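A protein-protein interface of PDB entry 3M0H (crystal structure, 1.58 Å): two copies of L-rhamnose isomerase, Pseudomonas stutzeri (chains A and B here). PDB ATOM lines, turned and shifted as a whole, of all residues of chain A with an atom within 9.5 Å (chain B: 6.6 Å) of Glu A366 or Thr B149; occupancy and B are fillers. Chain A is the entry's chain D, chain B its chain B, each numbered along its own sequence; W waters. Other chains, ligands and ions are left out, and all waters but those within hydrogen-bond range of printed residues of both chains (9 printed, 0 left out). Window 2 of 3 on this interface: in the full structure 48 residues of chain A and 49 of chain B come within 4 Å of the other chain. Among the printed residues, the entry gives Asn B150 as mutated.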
ATOM      1  N   ARG A 358      21.710  11.148  -4.366  1.00  0.00           N
ATOM      2  CA  ARG A 358      21.172  10.820  -5.684  1.00  0.00           C
ATOM      3  C   ARG A 358      22.067   9.905  -6.515  1.00  0.00           C
ATOM      4  O   ARG A 358      21.571   9.043  -7.243  1.00  0.00           O
ATOM      5  CB  ARG A 358      20.876  12.110  -6.456  1.00  0.00           C
ATOM      6  CG  ARG A 358      19.862  13.025  -5.768  1.00  0.00           C
ATOM      7  CD  ARG A 358      18.467  12.419  -5.774  1.00  0.00           C
ATOM      8  NE  ARG A 358      17.590  13.030  -4.776  1.00  0.00           N
ATOM      9  CZ  ARG A 358      16.367  12.589  -4.496  1.00  0.00           C
ATOM     10  NH1 ARG A 358      15.877  11.541  -5.145  1.00  0.00           N
ATOM     11  NH2 ARG A 358      15.644  13.176  -3.551  1.00  0.00           N
ATOM     12  N   ALA A 359      23.380  10.089  -6.412  1.00  0.00           N
ATOM     13  CA  ALA A 359      24.314   9.262  -7.169  1.00  0.00           C
ATOM     14  C   ALA A 359      24.246   7.820  -6.685  1.00  0.00           C
ATOM     15  O   ALA A 359      24.178   6.887  -7.486  1.00  0.00           O
ATOM     16  CB  ALA A 359      25.729   9.797  -7.018  1.00  0.00           C
ATOM     17  N   ALA A 360      24.265   7.644  -5.368  1.00  0.00           N
ATOM     18  CA  ALA A 360      24.198   6.312  -4.782  1.00  0.00           C
ATOM     19  C   ALA A 360      22.869   5.647  -5.118  1.00  0.00           C
ATOM     20  O   ALA A 360      22.830   4.475  -5.491  1.00  0.00           O
ATOM     21  CB  ALA A 360      24.370   6.393  -3.274  1.00  0.00           C
ATOM     22  N   LEU A 361      21.781   6.398  -4.985  1.00  0.00           N
ATOM     23  CA  LEU A 361      20.459   5.858  -5.275  1.00  0.00           C
ATOM     24  C   LEU A 361      20.364   5.391  -6.724  1.00  0.00           C
ATOM     25  O   LEU A 361      19.863   4.301  -6.998  1.00  0.00           O
ATOM     26  CB  LEU A 361      19.379   6.906  -4.997  1.00  0.00           C
ATOM     27  CG  LEU A 361      17.932   6.466  -5.252  1.00  0.00           C
ATOM     28  CD1 LEU A 361      17.576   5.277  -4.364  1.00  0.00           C
ATOM     29  CD2 LEU A 361      16.999   7.632  -4.974  1.00  0.00           C
ATOM     30  N   SER A 362      20.853   6.211  -7.650  1.00  0.00           N
ATOM     31  CA  SER A 362      20.811   5.856  -9.067  1.00  0.00           C
ATOM     32  C   SER A 362      21.574   4.560  -9.316  1.00  0.00           C
ATOM     33  O   SER A 362      21.153   3.723 -10.116  1.00  0.00           O
ATOM     34  CB  SER A 362      21.417   6.976  -9.913  1.00  0.00           C
ATOM     35  OG  SER A 362      20.681   8.175  -9.758  1.00  0.00           O
ATOM     36  N   GLY A 363      22.701   4.402  -8.630  1.00  0.00           N
ATOM     37  CA  GLY A 363      23.490   3.198  -8.795  1.00  0.00           C
ATOM     38  C   GLY A 363      22.732   1.966  -8.335  1.00  0.00           C
ATOM     39  O   GLY A 363      22.715   0.945  -9.020  1.00  0.00           O
ATOM     40  N   TYR A 364      22.093   2.060  -7.173  1.00  0.00           N
ATOM     41  CA  TYR A 364      21.343   0.930  -6.643  1.00  0.00           C
ATOM     42  C   TYR A 364      20.102   0.635  -7.472  1.00  0.00           C
ATOM     43  O   TYR A 364      19.652  -0.507  -7.536  1.00  0.00           O
ATOM     44  CB  TYR A 364      20.954   1.180  -5.182  1.00  0.00           C
ATOM     45  CG  TYR A 364      22.136   1.249  -4.241  1.00  0.00           C
ATOM     46  CD1 TYR A 364      23.094   0.234  -4.217  1.00  0.00           C
ATOM     47  CD2 TYR A 364      22.291   2.321  -3.364  1.00  0.00           C
ATOM     48  CE1 TYR A 364      24.175   0.285  -3.342  1.00  0.00           C
ATOM     49  CE2 TYR A 364      23.370   2.381  -2.482  1.00  0.00           C
ATOM     50  CZ  TYR A 364      24.306   1.360  -2.478  1.00  0.00           C
ATOM     51  OH  TYR A 364      25.370   1.412  -1.607  1.00  0.00           O
ATOM     52  N   GLN A 365      19.547   1.660  -8.108  1.00  0.00           N
ATOM     53  CA  GLN A 365      18.371   1.451  -8.944  1.00  0.00           C
ATOM     54  C   GLN A 365      18.787   0.705 -10.213  1.00  0.00           C
ATOM     55  O   GLN A 365      18.150  -0.271 -10.602  1.00  0.00           O
ATOM     56  CB  GLN A 365      17.714   2.792  -9.292  1.00  0.00           C
ATOM     57  CG  GLN A 365      17.120   3.501  -8.074  1.00  0.00           C
ATOM     58  CD  GLN A 365      16.521   4.857  -8.395  1.00  0.00           C
ATOM     59  OE1 GLN A 365      16.986   5.560  -9.292  1.00  0.00           O
ATOM     60  NE2 GLN A 365      15.498   5.241  -7.641  1.00  0.00           N
ATOM     61  N   GLU A 366      19.864   1.152 -10.850  1.00  0.00           N
ATOM     62  CA  GLU A 366      20.331   0.495 -12.068  1.00  0.00           C
ATOM     63  C   GLU A 366      20.746  -0.954 -11.822  1.00  0.00           C
ATOM     64  O   GLU A 366      20.525  -1.823 -12.666  1.00  0.00           O
ATOM     65  CB  GLU A 366      21.497   1.280 -12.678  1.00  0.00           C
ATOM     66  CG  GLU A 366      21.101   2.679 -13.110  1.00  0.00           C
ATOM     67  CD  GLU A 366      20.000   2.671 -14.156  1.00  0.00           C
ATOM     68  OE1 GLU A 366      19.234   3.656 -14.223  1.00  0.00           O
ATOM     69  OE2 GLU A 366      19.905   1.683 -14.917  1.00  0.00           O
ATOM     70  N   ASP A 367      21.331  -1.213 -10.656  1.00  0.00           N
ATOM     71  CA  ASP A 367      21.782  -2.556 -10.304  1.00  0.00           C
ATOM     72  C   ASP A 367      20.704  -3.412  -9.648  1.00  0.00           C
ATOM     73  O   ASP A 367      20.955  -4.551  -9.259  1.00  0.00           O
ATOM     74  CB  ASP A 367      22.999  -2.462  -9.384  1.00  0.00           C
ATOM     75  CG  ASP A 367      24.222  -1.917 -10.095  1.00  0.00           C
ATOM     76  OD1 ASP A 367      25.218  -1.600  -9.414  1.00  0.00           O
ATOM     77  OD2 ASP A 367      24.188  -1.813 -11.342  1.00  0.00           O
ATOM     78  N   ASN A 368      19.501  -2.862  -9.534  1.00  0.00           N
ATOM     79  CA  ASN A 368      18.390  -3.581  -8.926  1.00  0.00           C
ATOM     80  C   ASN A 368      18.685  -4.060  -7.509  1.00  0.00           C
ATOM     81  O   ASN A 368      18.287  -5.157  -7.115  1.00  0.00           O
ATOM     82  CB  ASN A 368      17.984  -4.759  -9.812  1.00  0.00           C
ATOM     83  CG  ASN A 368      17.369  -4.306 -11.122  1.00  0.00           C
ATOM     84  OD1 ASN A 368      17.897  -4.578 -12.204  1.00  0.00           O
ATOM     85  ND2 ASN A 368      16.251  -3.599 -11.029  1.00  0.00           N
ATOM     86  N   ASP A 369      19.394  -3.227  -6.752  1.00  0.00           N
ATOM     87  CA  ASP A 369      19.717  -3.524  -5.360  1.00  0.00           C
ATOM     88  C   ASP A 369      18.618  -2.811  -4.578  1.00  0.00           C
ATOM     89  O   ASP A 369      18.813  -1.707  -4.073  1.00  0.00           O
ATOM     90  CB  ASP A 369      21.083  -2.936  -5.004  1.00  0.00           C
ATOM     91  CG  ASP A 369      21.581  -3.384  -3.645  1.00  0.00           C
ATOM     92  OD1 ASP A 369      20.763  -3.847  -2.821  1.00  0.00           O
ATOM     93  OD2 ASP A 369      22.798  -3.259  -3.400  1.00  0.00           O
ATOM     94  N   ALA A 370      17.455  -3.452  -4.499  1.00  0.00           N
ATOM     95  CA  ALA A 370      16.293  -2.875  -3.830  1.00  0.00           C
ATOM     96  C   ALA A 370      16.525  -2.503  -2.375  1.00  0.00           C
ATOM     97  O   ALA A 370      16.080  -1.444  -1.918  1.00  0.00           O
ATOM     98  CB  ALA A 370      15.107  -3.833  -3.938  1.00  0.00           C
ATOM     99  N   ALA A 373      18.775   0.526  -2.148  1.00  0.00           N
ATOM    100  CA  ALA A 373      18.084   1.670  -2.726  1.00  0.00           C
ATOM    101  C   ALA A 373      17.139   2.252  -1.679  1.00  0.00           C
ATOM    102  O   ALA A 373      17.117   3.459  -1.452  1.00  0.00           O
ATOM    103  CB  ALA A 373      17.298   1.248  -3.965  1.00  0.00           C
ATOM    104  N   TYR B 143      13.249  -8.590 -11.648  1.00  0.00           N
ATOM    105  CA  TYR B 143      13.204  -7.148 -11.416  1.00  0.00           C
ATOM    106  C   TYR B 143      12.513  -6.362 -12.521  1.00  0.00           C
ATOM    107  O   TYR B 143      12.698  -5.150 -12.640  1.00  0.00           O
ATOM    108  CB  TYR B 143      14.624  -6.611 -11.224  1.00  0.00           C
ATOM    109  CG  TYR B 143      15.356  -7.246 -10.065  1.00  0.00           C
ATOM    110  CD1 TYR B 143      14.893  -7.097  -8.758  1.00  0.00           C
ATOM    111  CD2 TYR B 143      16.509  -7.999 -10.275  1.00  0.00           C
ATOM    112  CE1 TYR B 143      15.566  -7.683  -7.685  1.00  0.00           C
ATOM    113  CE2 TYR B 143      17.189  -8.588  -9.212  1.00  0.00           C
ATOM    114  CZ  TYR B 143      16.712  -8.428  -7.923  1.00  0.00           C
ATOM    115  OH  TYR B 143      17.382  -9.018  -6.874  1.00  0.00           O
ATOM    116  N   GLY B 144      11.717  -7.049 -13.329  1.00  0.00           N
ATOM    117  CA  GLY B 144      11.015  -6.367 -14.399  1.00  0.00           C
ATOM    118  C   GLY B 144      11.192  -7.047 -15.738  1.00  0.00           C
ATOM    119  O   GLY B 144      11.918  -8.033 -15.866  1.00  0.00           O
ATOM    120  N   SER B 145      10.520  -6.508 -16.747  1.00  0.00           N
ATOM    121  CA  SER B 145      10.590  -7.068 -18.084  1.00  0.00           C
ATOM    122  C   SER B 145      10.701  -5.945 -19.107  1.00  0.00           C
ATOM    123  O   SER B 145      11.803  -5.511 -19.440  1.00  0.00           O
ATOM    124  CB  SER B 145       9.354  -7.938 -18.348  1.00  0.00           C
ATOM    125  OG  SER B 145       8.150  -7.231 -18.095  1.00  0.00           O
ATOM    126  N   SER B 147      10.187  -2.939 -18.701  1.00  0.00           N
ATOM    127  CA  SER B 147      10.741  -1.737 -18.080  1.00  0.00           C
ATOM    128  C   SER B 147      11.982  -2.028 -17.236  1.00  0.00           C
ATOM    129  O   SER B 147      12.426  -1.181 -16.459  1.00  0.00           O
ATOM    130  CB  SER B 147       9.680  -1.046 -17.212  1.00  0.00           C
ATOM    131  OG  SER B 147       9.355  -1.813 -16.065  1.00  0.00           O
ATOM    132  N   HIS B 148      12.534  -3.226 -17.396  1.00  0.00           N
ATOM    133  CA  HIS B 148      13.726  -3.631 -16.656  1.00  0.00           C
ATOM    134  C   HIS B 148      14.875  -2.668 -16.971  1.00  0.00           C
ATOM    135  O   HIS B 148      14.937  -2.109 -18.070  1.00  0.00           O
ATOM    136  CB  HIS B 148      14.101  -5.065 -17.056  1.00  0.00           C
ATOM    137  CG  HIS B 148      15.068  -5.733 -16.127  1.00  0.00           C
ATOM    138  ND1 HIS B 148      16.403  -5.393 -16.066  1.00  0.00           N
ATOM    139  CD2 HIS B 148      14.897  -6.745 -15.244  1.00  0.00           C
ATOM    140  CE1 HIS B 148      17.013  -6.169 -15.187  1.00  0.00           C
ATOM    141  NE2 HIS B 148      16.122  -6.998 -14.673  1.00  0.00           N
ATOM    142  N   THR B 149      15.773  -2.466 -16.011  1.00  0.00           N
ATOM    143  CA  THR B 149      16.900  -1.570 -16.235  1.00  0.00           C
ATOM    144  C   THR B 149      17.897  -2.128 -17.241  1.00  0.00           C
ATOM    145  O   THR B 149      18.639  -1.370 -17.863  1.00  0.00           O
ATOM    146  CB  THR B 149      17.655  -1.271 -14.926  1.00  0.00           C
ATOM    147  OG1 THR B 149      18.116  -2.499 -14.361  1.00  0.00           O
ATOM    148  CG2 THR B 149      16.750  -0.570 -13.933  1.00  0.00           C
ATOM    149  N   ASN B 150      17.916  -3.445 -17.413  1.00  0.00           N
ATOM    150  CA  ASN B 150      18.862  -4.074 -18.340  1.00  0.00           C
ATOM    151  C   ASN B 150      18.287  -4.085 -19.758  1.00  0.00           C
ATOM    152  O   ASN B 150      17.208  -4.624 -20.001  1.00  0.00           O
ATOM    153  CB  ASN B 150      19.141  -5.487 -17.846  1.00  0.00           C
ATOM    154  CG  ASN B 150      20.246  -6.187 -18.616  1.00  0.00           C
ATOM    155  OD1 ASN B 150      21.375  -5.701 -18.733  1.00  0.00           O
ATOM    156  ND2 ASN B 150      19.917  -7.356 -19.146  1.00  0.00           N
ATOM    157  N   ALA B 151      19.027  -3.486 -20.689  1.00  0.00           N
ATOM    158  CA  ALA B 151      18.603  -3.395 -22.085  1.00  0.00           C
ATOM    159  C   ALA B 151      18.305  -4.753 -22.702  1.00  0.00           C
ATOM    160  O   ALA B 151      17.288  -4.923 -23.374  1.00  0.00           O
ATOM    161  CB  ALA B 151      19.678  -2.667 -22.910  1.00  0.00           C
ATOM    162  N   ALA B 152      19.190  -5.718 -22.474  1.00  0.00           N
ATOM    163  CA  ALA B 152      19.014  -7.057 -23.023  1.00  0.00           C
ATOM    164  C   ALA B 152      17.751  -7.731 -22.500  1.00  0.00           C
ATOM    165  O   ALA B 152      17.112  -8.507 -23.210  1.00  0.00           O
ATOM    166  CB  ALA B 152      20.230  -7.909 -22.702  1.00  0.00           C
ATOM    167  N   THR B 153      17.390  -7.428 -21.258  1.00  0.00           N
ATOM    168  CA  THR B 153      16.197  -8.014 -20.665  1.00  0.00           C
ATOM    169  C   THR B 153      14.958  -7.417 -21.320  1.00  0.00           C
ATOM    170  O   THR B 153      13.999  -8.128 -21.607  1.00  0.00           O
ATOM    171  CB  THR B 153      16.159  -7.777 -19.143  1.00  0.00           C
ATOM    172  OG1 THR B 153      17.334  -8.347 -18.552  1.00  0.00           O
ATOM    173  CG2 THR B 153      14.934  -8.436 -18.526  1.00  0.00           C
ATOM    174  N   ARG B 154      14.983  -6.112 -21.566  1.00  0.00           N
ATOM    175  CA  ARG B 154      13.848  -5.464 -22.212  1.00  0.00           C
ATOM    176  C   ARG B 154      13.701  -6.010 -23.632  1.00  0.00           C
ATOM    177  O   ARG B 154      12.590  -6.269 -24.095  1.00  0.00           O
ATOM    178  CB  ARG B 154      14.038  -3.943 -22.253  1.00  0.00           C
ATOM    179  CG  ARG B 154      14.110  -3.284 -20.877  1.00  0.00           C
ATOM    180  CD  ARG B 154      13.867  -1.781 -20.960  1.00  0.00           C
ATOM    181  NE  ARG B 154      14.849  -1.077 -21.779  1.00  0.00           N
ATOM    182  CZ  ARG B 154      16.091  -0.799 -21.395  1.00  0.00           C
ATOM    183  NH1 ARG B 154      16.518  -1.163 -20.193  1.00  0.00           N
ATOM    184  NH2 ARG B 154      16.907  -0.145 -22.213  1.00  0.00           N
ATOM    185  N   GLN B 189      13.525   1.756  -4.769  1.00  0.00           N
ATOM    186  CA  GLN B 189      13.970   0.644  -5.607  1.00  0.00           C
ATOM    187  C   GLN B 189      13.925   1.014  -7.088  1.00  0.00           C
ATOM    188  O   GLN B 189      14.849   0.701  -7.843  1.00  0.00           O
ATOM    189  CB  GLN B 189      13.103  -0.597  -5.358  1.00  0.00           C
ATOM    190  CG  GLN B 189      13.386  -1.741  -6.326  1.00  0.00           C
ATOM    191  CD  GLN B 189      12.501  -2.954  -6.095  1.00  0.00           C
ATOM    192  OE1 GLN B 189      12.556  -3.927  -6.852  1.00  0.00           O
ATOM    193  NE2 GLN B 189      11.685  -2.906  -5.052  1.00  0.00           N
ATOM    194  N   ARG B 194      11.751   7.065 -14.869  1.00  0.00           N
ATOM    195  CA  ARG B 194      12.643   6.334 -15.760  1.00  0.00           C
ATOM    196  C   ARG B 194      12.093   4.958 -16.110  1.00  0.00           C
ATOM    197  O   ARG B 194      12.219   4.504 -17.247  1.00  0.00           O
ATOM    198  CB  ARG B 194      14.038   6.238 -15.140  1.00  0.00           C
ATOM    199  CG  ARG B 194      14.758   7.575 -15.200  1.00  0.00           C
ATOM    200  CD  ARG B 194      16.030   7.610 -14.382  1.00  0.00           C
ATOM    201  NE  ARG B 194      16.702   8.896 -14.543  1.00  0.00           N
ATOM    202  CZ  ARG B 194      17.517   9.433 -13.642  1.00  0.00           C
ATOM    203  NH1 ARG B 194      17.761   8.796 -12.505  1.00  0.00           N
ATOM    204  NH2 ARG B 194      18.085  10.609 -13.878  1.00  0.00           N
ATOM    205  N   ARG B 198      11.222   3.659 -19.879  1.00  0.00           N
ATOM    206  CA  ARG B 198      11.712   2.406 -20.447  1.00  0.00           C
ATOM    207  C   ARG B 198      10.537   1.587 -20.975  1.00  0.00           C
ATOM    208  O   ARG B 198      10.614   0.994 -22.051  1.00  0.00           O
ATOM    209  CB  ARG B 198      12.495   1.600 -19.398  1.00  0.00           C
ATOM    210  CG  ARG B 198      13.808   2.252 -18.967  1.00  0.00           C
ATOM    211  CD  ARG B 198      14.671   1.295 -18.144  1.00  0.00           C
ATOM    212  NE  ARG B 198      14.123   0.999 -16.821  1.00  0.00           N
ATOM    213  CZ  ARG B 198      14.328   1.739 -15.734  1.00  0.00           C
ATOM    214  NH1 ARG B 198      15.072   2.835 -15.800  1.00  0.00           N
ATOM    215  NH2 ARG B 198      13.804   1.370 -14.572  1.00  0.00           N
HETATM  216  O   HOH W   1      16.442   3.815 -13.355  1.00  0.00           O
HETATM  217  O   HOH W   2      17.444  -6.539  -4.727  1.00  0.00           O
HETATM  218  O   HOH W   3      13.874  -3.484  -9.446  1.00  0.00           O
HETATM  219  O   HOH W   4      20.695  -3.046 -15.301  1.00  0.00           O
HETATM  220  O   HOH W   5      17.373   6.090 -12.013  1.00  0.00           O
HETATM  221  O   HOH W   6      15.501   0.236 -10.467  1.00  0.00           O
HETATM  222  O   HOH W   7      16.726  -1.284  -7.008  1.00  0.00           O
HETATM  223  O   HOH W   8      14.768  -3.374 -13.292  1.00  0.00           O
HETATM  224  O   HOH W   9      18.311   1.441 -17.392  1.00  0.00           O
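The side-chain hydroxyl of Thr B149 lies within hydrogen-bond range of the side-chain amide oxygen of Asn A368 (3.0 Å). O of Glu A366 sits at hydrogen-bond distance from OG1 of Thr B149 (3.0 Å).
The backbone carbonyl oxygen (O) of Thr B149 sits at hydrogen-bond distance from the guanidinium group (NH1) of Arg B154, 3.2 Å away. A ring nitrogen (ND1) of His B148 sits at hydrogen-bond distance from the backbone NH (N) of Asn B150, 2.8 Å away. NH1 of Arg B154 sits at hydrogen-bond distance from O of His B148, 2.8 Å away. The backbone carbonyl oxygen (O) of His B148 sits close to the guanidinium group (NE) of Arg B198, 3.4 Å away.
Water W6 lies within hydrogen-bond range of O of Gln A365 (2.7 Å) and O of Gln B189 (2.7 Å). Water W8 lies within hydrogen-bond range of the side-chain amide nitrogen (ND2) of Asn A368 (2.7 Å), the backbone carbonyl oxygen (O) of Tyr B143 (2.8 Å) and the backbone NH (N) of Thr B149 (3.0 Å). Water W5 lies within hydrogen-bond range of NH1 of Arg B194 and OE1 of Gln A365. Water W4 bridges OG1 of Thr B149 (2.8 Å) and O of Glu A366 (2.9 Å). Water W3 bridges the side-chain amide nitrogen (ND2) of Asn A368 (2.9 Å) and the side-chain amide oxygen (OE1) of Gln B189 (2.9 Å). Water W1 bridges OE1 of Glu A366 and NH1 of Arg B198.
Among the printed residues, merely in contact across the chains: Asn A368 with Tyr B143, Asn A368 with His B148, Ala A370 with Gln B189, Gln A365 with Gln B189, Gln A365 with Thr B149 and Ala A373 with Gln B189.
No position is printed for both chains. Of the 8 pairs that touch across the chains among the printed residues, none has its exchanged pair printed and touching as well.
Leu A361 touches none of the printed residues of chain B. Printed residues of chain B within 4 Å of Glu A366: Thr B149 (3.0 Å). Of the printed residues of chain B, Asn A368 touches Tyr B143 (3.4 Å), His B148 (3.5 Å) and Thr B149 (3.0 Å). Of the printed residues of chain A, Tyr B143 touches Asn A368. His B148 touches just one residue of chain A: Asn A368 (3.5 Å). Thr B149 touches just these residues of chain A: Gln A365, Glu A366 and Asn A368. Printed residues of chain A within 4 Å of Gln B189: Gln A365 (3.6 Å), Ala A370 (3.5 Å) and Ala A373 (3.8 Å). The nearest printed residue of chain A that does not touch Gln B189 is Tyr A364 (5.0 Å).
Of the 14 printed residues of chain B, 4 touch a printed residue of chain A. Printed residues of chain B that touch a printed residue of chain A: Tyr B143, His B148, Thr B149 and Gln B189. Along chain B the printed residues that touch a printed residue of chain A span positions 143 to 189. Among the printed residues, no Asp or Glu carboxylate lies within 4 Å of a Lys or Arg side-chain nitrogen of the other chain.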
